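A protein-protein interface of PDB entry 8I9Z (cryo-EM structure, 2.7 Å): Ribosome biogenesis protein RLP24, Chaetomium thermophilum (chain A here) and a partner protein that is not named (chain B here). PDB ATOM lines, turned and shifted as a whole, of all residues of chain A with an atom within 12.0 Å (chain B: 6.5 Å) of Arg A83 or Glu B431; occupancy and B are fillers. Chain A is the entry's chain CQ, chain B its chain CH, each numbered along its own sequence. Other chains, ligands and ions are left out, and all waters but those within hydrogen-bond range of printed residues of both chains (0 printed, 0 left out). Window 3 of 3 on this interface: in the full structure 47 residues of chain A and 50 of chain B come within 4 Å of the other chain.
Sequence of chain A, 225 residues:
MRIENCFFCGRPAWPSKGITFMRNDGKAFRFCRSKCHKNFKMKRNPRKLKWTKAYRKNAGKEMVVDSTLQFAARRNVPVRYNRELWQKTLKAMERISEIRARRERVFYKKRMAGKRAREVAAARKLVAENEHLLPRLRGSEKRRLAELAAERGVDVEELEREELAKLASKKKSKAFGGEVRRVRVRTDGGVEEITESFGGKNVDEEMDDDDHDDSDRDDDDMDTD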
ATOM      1  N   VAL A  79      28.170  33.928 -31.995  1.00  0.00           N
ATOM      2  CA  VAL A  79      27.181  32.861 -32.011  1.00  0.00           C
ATOM      3  C   VAL A  79      26.482  32.850 -30.662  1.00  0.00           C
ATOM      4  O   VAL A  79      27.002  33.359 -29.662  1.00  0.00           O
ATOM      5  CB  VAL A  79      27.793  31.477 -32.323  1.00  0.00           C
ATOM      6  CG1 VAL A  79      28.637  31.541 -33.581  1.00  0.00           C
ATOM      7  CG2 VAL A  79      28.596  30.961 -31.148  1.00  0.00           C
ATOM      8  N   ARG A  80      25.272  32.303 -30.648  1.00  0.00           N
ATOM      9  CA  ARG A  80      24.576  32.087 -29.392  1.00  0.00           C
ATOM     10  C   ARG A  80      25.310  31.022 -28.593  1.00  0.00           C
ATOM     11  O   ARG A  80      25.883  30.089 -29.161  1.00  0.00           O
ATOM     12  CB  ARG A  80      23.132  31.662 -29.654  1.00  0.00           C
ATOM     13  CG  ARG A  80      22.221  31.743 -28.446  1.00  0.00           C
ATOM     14  CD  ARG A  80      20.800  32.064 -28.849  1.00  0.00           C
ATOM     15  NE  ARG A  80      20.711  33.283 -29.637  1.00  0.00           N
ATOM     16  CZ  ARG A  80      20.307  34.451 -29.160  1.00  0.00           C
ATOM     17  NH1 ARG A  80      19.945  34.592 -27.897  1.00  0.00           N
ATOM     18  NH2 ARG A  80      20.266  35.503 -29.971  1.00  0.00           N
ATOM     19  N   TYR A  81      25.321  31.180 -27.271  1.00  0.00           N
ATOM     20  CA  TYR A  81      26.017  30.221 -26.426  1.00  0.00           C
ATOM     21  C   TYR A  81      25.340  28.863 -26.493  1.00  0.00           C
ATOM     22  O   TYR A  81      24.114  28.751 -26.432  1.00  0.00           O
ATOM     23  CB  TYR A  81      26.074  30.701 -24.977  1.00  0.00           C
ATOM     24  CG  TYR A  81      26.637  29.654 -24.045  1.00  0.00           C
ATOM     25  CD1 TYR A  81      27.973  29.293 -24.104  1.00  0.00           C
ATOM     26  CD2 TYR A  81      25.829  29.016 -23.117  1.00  0.00           C
ATOM     27  CE1 TYR A  81      28.488  28.331 -23.267  1.00  0.00           C
ATOM     28  CE2 TYR A  81      26.338  28.055 -22.273  1.00  0.00           C
ATOM     29  CZ  TYR A  81      27.668  27.716 -22.353  1.00  0.00           C
ATOM     30  OH  TYR A  81      28.182  26.760 -21.514  1.00  0.00           O
ATOM     31  N   ASN A  82      26.159  27.829 -26.627  1.00  0.00           N
ATOM     32  CA  ASN A  82      25.664  26.465 -26.754  1.00  0.00           C
ATOM     33  C   ASN A  82      26.672  25.583 -26.035  1.00  0.00           C
ATOM     34  O   ASN A  82      27.837  25.528 -26.442  1.00  0.00           O
ATOM     35  CB  ASN A  82      25.518  26.091 -28.225  1.00  0.00           C
ATOM     36  CG  ASN A  82      24.843  24.757 -28.435  1.00  0.00           C
ATOM     37  OD1 ASN A  82      24.476  24.075 -27.489  1.00  0.00           O
ATOM     38  ND2 ASN A  82      24.669  24.382 -29.694  1.00  0.00           N
ATOM     39  N   ARG A  83      26.235  24.926 -24.957  1.00  0.00           N
ATOM     40  CA  ARG A  83      27.154  24.137 -24.145  1.00  0.00           C
ATOM     41  C   ARG A  83      27.705  22.951 -24.925  1.00  0.00           C
ATOM     42  O   ARG A  83      28.869  22.571 -24.751  1.00  0.00           O
ATOM     43  CB  ARG A  83      26.465  23.657 -22.869  1.00  0.00           C
ATOM     44  CG  ARG A  83      27.441  23.086 -21.854  1.00  0.00           C
ATOM     45  CD  ARG A  83      26.756  22.332 -20.740  1.00  0.00           C
ATOM     46  NE  ARG A  83      26.016  23.213 -19.848  1.00  0.00           N
ATOM     47  CZ  ARG A  83      25.182  22.792 -18.908  1.00  0.00           C
ATOM     48  NH1 ARG A  83      24.959  21.505 -18.710  1.00  0.00           N
ATOM     49  NH2 ARG A  83      24.556  23.685 -18.149  1.00  0.00           N
ATOM     50  N   GLU A  84      26.880  22.349 -25.781  1.00  0.00           N
ATOM     51  CA  GLU A  84      27.355  21.244 -26.605  1.00  0.00           C
ATOM     52  C   GLU A  84      28.383  21.717 -27.623  1.00  0.00           C
ATOM     53  O   GLU A  84      29.337  20.994 -27.931  1.00  0.00           O
ATOM     54  CB  GLU A  84      26.178  20.565 -27.302  1.00  0.00           C
ATOM     55  CG  GLU A  84      25.091  20.095 -26.353  1.00  0.00           C
ATOM     56  CD  GLU A  84      25.298  18.662 -25.897  1.00  0.00           C
ATOM     57  OE1 GLU A  84      26.342  18.070 -26.241  1.00  0.00           O
ATOM     58  OE2 GLU A  84      24.416  18.127 -25.193  1.00  0.00           O
ATOM     59  N   LEU A  85      28.205  22.927 -28.157  1.00  0.00           N
ATOM     60  CA  LEU A  85      29.169  23.462 -29.111  1.00  0.00           C
ATOM     61  C   LEU A  85      30.487  23.815 -28.436  1.00  0.00           C
ATOM     62  O   LEU A  85      31.560  23.611 -29.014  1.00  0.00           O
ATOM     63  CB  LEU A  85      28.589  24.684 -29.817  1.00  0.00           C
ATOM     64  CG  LEU A  85      29.427  25.263 -30.955  1.00  0.00           C
ATOM     65  CD1 LEU A  85      29.823  24.183 -31.947  1.00  0.00           C
ATOM     66  CD2 LEU A  85      28.690  26.394 -31.644  1.00  0.00           C
ATOM     67  N   TRP A  86      30.431  24.349 -27.214  1.00  0.00           N
ATOM     68  CA  TRP A  86      31.657  24.769 -26.538  1.00  0.00           C
ATOM     69  C   TRP A  86      32.473  23.580 -26.054  1.00  0.00           C
ATOM     70  O   TRP A  86      33.706  23.638 -26.028  1.00  0.00           O
ATOM     71  CB  TRP A  86      31.329  25.700 -25.373  1.00  0.00           C
ATOM     72  CG  TRP A  86      31.683  27.118 -25.645  1.00  0.00           C
ATOM     73  CD1 TRP A  86      32.758  27.796 -25.166  1.00  0.00           C
ATOM     74  CD2 TRP A  86      30.970  28.034 -26.477  1.00  0.00           C
ATOM     75  NE1 TRP A  86      32.758  29.081 -25.641  1.00  0.00           N
ATOM     76  CE2 TRP A  86      31.667  29.252 -26.449  1.00  0.00           C
ATOM     77  CE3 TRP A  86      29.805  27.941 -27.240  1.00  0.00           C
ATOM     78  CZ2 TRP A  86      31.239  30.369 -27.154  1.00  0.00           C
ATOM     79  CZ3 TRP A  86      29.382  29.050 -27.938  1.00  0.00           C
ATOM     80  CH2 TRP A  86      30.097  30.247 -27.890  1.00  0.00           C
ATOM     81  N   GLN A  87      31.809  22.498 -25.641  1.00  0.00           N
ATOM     82  CA  GLN A  87      32.543  21.303 -25.239  1.00  0.00           C
ATOM     83  C   GLN A  87      33.178  20.622 -26.444  1.00  0.00           C
ATOM     84  O   GLN A  87      34.321  20.159 -26.380  1.00  0.00           O
ATOM     85  CB  GLN A  87      31.621  20.340 -24.497  1.00  0.00           C
ATOM     86  CG  GLN A  87      31.199  20.821 -23.125  1.00  0.00           C
ATOM     87  CD  GLN A  87      32.375  21.176 -22.240  1.00  0.00           C
ATOM     88  OE1 GLN A  87      32.527  22.325 -21.827  1.00  0.00           O
ATOM     89  NE2 GLN A  87      33.205  20.187 -21.925  1.00  0.00           N
ATOM     90  N   LYS A  88      32.451  20.557 -27.559  1.00  0.00           N
ATOM     91  CA  LYS A  88      33.004  19.916 -28.745  1.00  0.00           C
ATOM     92  C   LYS A  88      34.033  20.799 -29.433  1.00  0.00           C
ATOM     93  O   LYS A  88      34.842  20.303 -30.225  1.00  0.00           O
ATOM     94  CB  LYS A  88      31.883  19.541 -29.710  1.00  0.00           C
ATOM     95  CG  LYS A  88      31.322  20.697 -30.512  1.00  0.00           C
ATOM     96  CD  LYS A  88      30.328  20.294 -31.608  1.00  0.00           C
ATOM     97  CE  LYS A  88      29.534  18.997 -31.373  1.00  0.00           C
ATOM     98  NZ  LYS A  88      28.788  18.894 -30.076  1.00  0.00           N
ATOM     99  N   THR A  89      34.009  22.103 -29.161  1.00  0.00           N
ATOM    100  CA  THR A  89      35.068  22.977 -29.646  1.00  0.00           C
ATOM    101  C   THR A  89      36.380  22.668 -28.944  1.00  0.00           C
ATOM    102  O   THR A  89      37.443  22.665 -29.572  1.00  0.00           O
ATOM    103  CB  THR A  89      34.674  24.436 -29.437  1.00  0.00           C
ATOM    104  OG1 THR A  89      33.404  24.663 -30.053  1.00  0.00           O
ATOM    105  CG2 THR A  89      35.681  25.364 -30.078  1.00  0.00           C
ATOM    106  N   LEU A  90      36.315  22.369 -27.647  1.00  0.00           N
ATOM    107  CA  LEU A  90      37.520  22.115 -26.867  1.00  0.00           C
ATOM    108  C   LEU A  90      38.214  20.836 -27.310  1.00  0.00           C
ATOM    109  O   LEU A  90      39.447  20.765 -27.345  1.00  0.00           O
ATOM    110  CB  LEU A  90      37.168  22.043 -25.385  1.00  0.00           C
ATOM    111  CG  LEU A  90      36.837  23.358 -24.686  1.00  0.00           C
ATOM    112  CD1 LEU A  90      37.124  23.189 -23.227  1.00  0.00           C
ATOM    113  CD2 LEU A  90      37.630  24.522 -25.254  1.00  0.00           C
ATOM    114  N   LYS A  91      37.435  19.805 -27.643  1.00  0.00           N
ATOM    115  CA  LYS A  91      38.031  18.571 -28.139  1.00  0.00           C
ATOM    116  C   LYS A  91      38.623  18.766 -29.529  1.00  0.00           C
ATOM    117  O   LYS A  91      39.527  18.027 -29.935  1.00  0.00           O
ATOM    118  CB  LYS A  91      36.992  17.453 -28.152  1.00  0.00           C
ATOM    119  CG  LYS A  91      36.422  17.111 -26.789  1.00  0.00           C
ATOM    120  CD  LYS A  91      35.108  16.361 -26.933  1.00  0.00           C
ATOM    121  CE  LYS A  91      34.363  16.276 -25.613  1.00  0.00           C
ATOM    122  NZ  LYS A  91      32.975  15.769 -25.801  1.00  0.00           N
ATOM    123  N   ALA A  92      38.120  19.748 -30.276  1.00  0.00           N
ATOM    124  CA  ALA A  92      38.677  20.035 -31.591  1.00  0.00           C
ATOM    125  C   ALA A  92      40.067  20.646 -31.485  1.00  0.00           C
ATOM    126  O   ALA A  92      40.985  20.233 -32.203  1.00  0.00           O
ATOM    127  CB  ALA A  92      37.743  20.958 -32.370  1.00  0.00           C
ATOM    128  N   MET A  93      40.248  21.627 -30.595  1.00  0.00           N
ATOM    129  CA  MET A  93      41.545  22.285 -30.477  1.00  0.00           C
ATOM    130  C   MET A  93      42.609  21.385 -29.863  1.00  0.00           C
ATOM    131  O   MET A  93      43.802  21.628 -30.070  1.00  0.00           O
ATOM    132  CB  MET A  93      41.428  23.581 -29.670  1.00  0.00           C
ATOM    133  CG  MET A  93      40.129  24.321 -29.854  1.00  0.00           C
ATOM    134  SD  MET A  93      39.642  25.264 -28.399  1.00  0.00           S
ATOM    135  CE  MET A  93      41.079  26.301 -28.186  1.00  0.00           C
ATOM    136  N   LEU B 427      18.640  31.490 -24.719  1.00  0.00           N
ATOM    137  CA  LEU B 427      19.445  30.353 -25.128  1.00  0.00           C
ATOM    138  C   LEU B 427      18.525  29.226 -25.568  1.00  0.00           C
ATOM    139  O   LEU B 427      17.305  29.289 -25.406  1.00  0.00           O
ATOM    140  CB  LEU B 427      20.366  29.880 -23.997  1.00  0.00           C
ATOM    141  CG  LEU B 427      21.407  30.873 -23.483  1.00  0.00           C
ATOM    142  CD1 LEU B 427      22.173  30.288 -22.316  1.00  0.00           C
ATOM    143  CD2 LEU B 427      22.352  31.248 -24.601  1.00  0.00           C
ATOM    144  N   ASN B 429      18.639  26.163 -24.317  1.00  0.00           N
ATOM    145  CA  ASN B 429      18.265  25.470 -23.092  1.00  0.00           C
ATOM    146  C   ASN B 429      18.343  26.449 -21.931  1.00  0.00           C
ATOM    147  O   ASN B 429      19.397  27.078 -21.733  1.00  0.00           O
ATOM    148  CB  ASN B 429      19.180  24.269 -22.848  1.00  0.00           C
ATOM    149  CG  ASN B 429      18.666  23.347 -21.766  1.00  0.00           C
ATOM    150  OD1 ASN B 429      17.536  23.478 -21.303  1.00  0.00           O
ATOM    151  ND2 ASN B 429      19.499  22.400 -21.357  1.00  0.00           N
ATOM    152  N   PRO B 430      17.265  26.637 -21.160  1.00  0.00           N
ATOM    153  CA  PRO B 430      17.323  27.579 -20.028  1.00  0.00           C
ATOM    154  C   PRO B 430      18.308  27.188 -18.940  1.00  0.00           C
ATOM    155  O   PRO B 430      18.705  28.048 -18.146  1.00  0.00           O
ATOM    156  CB  PRO B 430      15.885  27.584 -19.497  1.00  0.00           C
ATOM    157  CG  PRO B 430      15.043  27.105 -20.609  1.00  0.00           C
ATOM    158  CD  PRO B 430      15.886  26.278 -21.527  1.00  0.00           C
ATOM    159  N   GLU B 431      18.709  25.919 -18.864  1.00  0.00           N
ATOM    160  CA  GLU B 431      19.709  25.519 -17.884  1.00  0.00           C
ATOM    161  C   GLU B 431      21.113  25.965 -18.270  1.00  0.00           C
ATOM    162  O   GLU B 431      22.010  25.950 -17.422  1.00  0.00           O
ATOM    163  CB  GLU B 431      19.681  24.002 -17.702  1.00  0.00           C
ATOM    164  CG  GLU B 431      18.700  23.521 -16.652  1.00  0.00           C
ATOM    165  CD  GLU B 431      19.102  22.191 -16.048  1.00  0.00           C
ATOM    166  OE1 GLU B 431      18.801  21.144 -16.659  1.00  0.00           O
ATOM    167  OE2 GLU B 431      19.718  22.190 -14.961  1.00  0.00           O
ATOM    168  N   TRP B 432      21.325  26.366 -19.527  1.00  0.00           N
ATOM    169  CA  TRP B 432      22.663  26.720 -19.987  1.00  0.00           C
ATOM    170  C   TRP B 432      23.088  28.109 -19.542  1.00  0.00           C
ATOM    171  O   TRP B 432      24.269  28.445 -19.664  1.00  0.00           O
ATOM    172  CB  TRP B 432      22.742  26.628 -21.507  1.00  0.00           C
ATOM    173  CG  TRP B 432      22.847  25.236 -21.994  1.00  0.00           C
ATOM    174  CD1 TRP B 432      23.217  24.147 -21.273  1.00  0.00           C
ATOM    175  CD2 TRP B 432      22.566  24.770 -23.314  1.00  0.00           C
ATOM    176  NE1 TRP B 432      23.189  23.026 -22.061  1.00  0.00           N
ATOM    177  CE2 TRP B 432      22.787  23.383 -23.320  1.00  0.00           C
ATOM    178  CE3 TRP B 432      22.141  25.390 -24.491  1.00  0.00           C
ATOM    179  CZ2 TRP B 432      22.608  22.607 -24.455  1.00  0.00           C
ATOM    180  CZ3 TRP B 432      21.958  24.618 -25.612  1.00  0.00           C
ATOM    181  CH2 TRP B 432      22.188  23.240 -25.587  1.00  0.00           C
ATOM    182  N   LYS B 433      22.168  28.929 -19.049  1.00  0.00           N
ATOM    183  CA  LYS B 433      22.592  30.167 -18.425  1.00  0.00           C
ATOM    184  C   LYS B 433      23.185  29.866 -17.053  1.00  0.00           C
ATOM    185  O   LYS B 433      23.089  28.748 -16.535  1.00  0.00           O
ATOM    186  CB  LYS B 433      21.434  31.155 -18.325  1.00  0.00           C
ATOM    187  CG  LYS B 433      20.347  30.745 -17.371  1.00  0.00           C
ATOM    188  CD  LYS B 433      19.287  31.823 -17.275  1.00  0.00           C
ATOM    189  CE  LYS B 433      18.552  31.995 -18.586  1.00  0.00           C
ATOM    190  NZ  LYS B 433      17.466  32.998 -18.454  1.00  0.00           N
ATOM    191  N   TYR B 434      23.809  30.889 -16.468  1.00  0.00           N
ATOM    192  CA  TYR B 434      24.678  30.770 -15.299  1.00  0.00           C
ATOM    193  C   TYR B 434      25.799  29.762 -15.524  1.00  0.00           C
ATOM    194  O   TYR B 434      26.156  29.010 -14.613  1.00  0.00           O
ATOM    195  CB  TYR B 434      23.898  30.424 -14.023  1.00  0.00           C
ATOM    196  CG  TYR B 434      22.644  31.237 -13.838  1.00  0.00           C
ATOM    197  CD1 TYR B 434      21.394  30.655 -13.961  1.00  0.00           C
ATOM    198  CD2 TYR B 434      22.711  32.592 -13.558  1.00  0.00           C
ATOM    199  CE1 TYR B 434      20.246  31.397 -13.798  1.00  0.00           C
ATOM    200  CE2 TYR B 434      21.571  33.340 -13.396  1.00  0.00           C
ATOM    201  CZ  TYR B 434      20.342  32.741 -13.519  1.00  0.00           C
ATOM    202  OH  TYR B 434      19.201  33.488 -13.354  1.00  0.00           O
ATOM    203  N   ASP B 435      26.350  29.723 -16.731  1.00  0.00           N
ATOM    204  CA  ASP B 435      27.457  28.836 -17.047  1.00  0.00           C
ATOM    205  C   ASP B 435      28.767  29.608 -17.102  1.00  0.00           C
ATOM    206  O   ASP B 435      28.809  30.792 -17.437  1.00  0.00           O
ATOM    207  CB  ASP B 435      27.226  28.121 -18.375  1.00  0.00           C
ATOM    208  CG  ASP B 435      26.629  26.743 -18.194  1.00  0.00           C
ATOM    209  OD1 ASP B 435      26.188  26.431 -17.071  1.00  0.00           O
ATOM    210  OD2 ASP B 435      26.600  25.971 -19.173  1.00  0.00           O
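The backbone carbonyl oxygen (O) of Glu B431 lies within hydrogen-bond range of the guanidinium group (NH2) of Arg A83 (3.5 Å).
The side-chain hydroxyl (OH) of Tyr A81 sits at hydrogen-bond distance from the side-chain carboxylate (OD2) of Asp B435 (2.9 Å).
The side-chain carboxylate (OD2) of Asp B435 is in salt-bridge range of the guanidinium group (NE) of Arg A83 (2.9 Å).
Of chain B, only Glu B431, Trp B432 and Asp B435 come within 4 Å of Arg A83.
Of chain A, only Arg A83 (3.5 Å) comes within 4 Å of Glu B431.
No residue of chain A comes within 4 Å of Asn B429.
No residue of chain A comes within 4 Å of Lys B433.
Of the printed residues of chain B, Arg A80 touches Leu B427.
Of the printed residues of chain B, Tyr A81 touches Leu B427 (3.6 Å), Trp B432 (3.4 Å) and Asp B435 (2.9 Å).
Of the printed residues of chain A, Trp B432 touches Tyr A81 (3.4 Å), Asn A82 (3.1 Å) and Arg A83 (3.3 Å).
Of the printed residues of chain B, Asn A82 touches Trp B432.
The nearest residue of chain A that does not touch Glu B431 is Tyr A81 (6.8 Å).
OD1 of Asn A82 sits close to N of Glu A84 (3.4 Å).
Of the 8 printed residues of chain B, 4 touch a printed residue of chain A.
Printed residues of chain B that touch a printed residue of chain A: Leu B427, Glu B431, Trp B432 and Asp B435.
Hydrophobic or aromatic side chains of chain B within 4 Å of the printed part of chain A: Leu B427 and Trp B432.
Among the printed residues, 8 pairs touch across the chains.
Among the printed residues, Asp or Glu carboxylates within 4 Å of a Lys or Arg side-chain nitrogen of the other chain: Arg A83 with Asp B435 (2.9 Å).
Among the printed residues, merely in contact across the chains: Arg A80 with Leu B427 (3.9 Å), Tyr A81 with Leu B427 (3.6 Å), Tyr A81 with Trp B432 (3.4 Å), Asn A82 with Trp B432 (3.1 Å) and Arg A83 with Trp B432 (3.3 Å).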
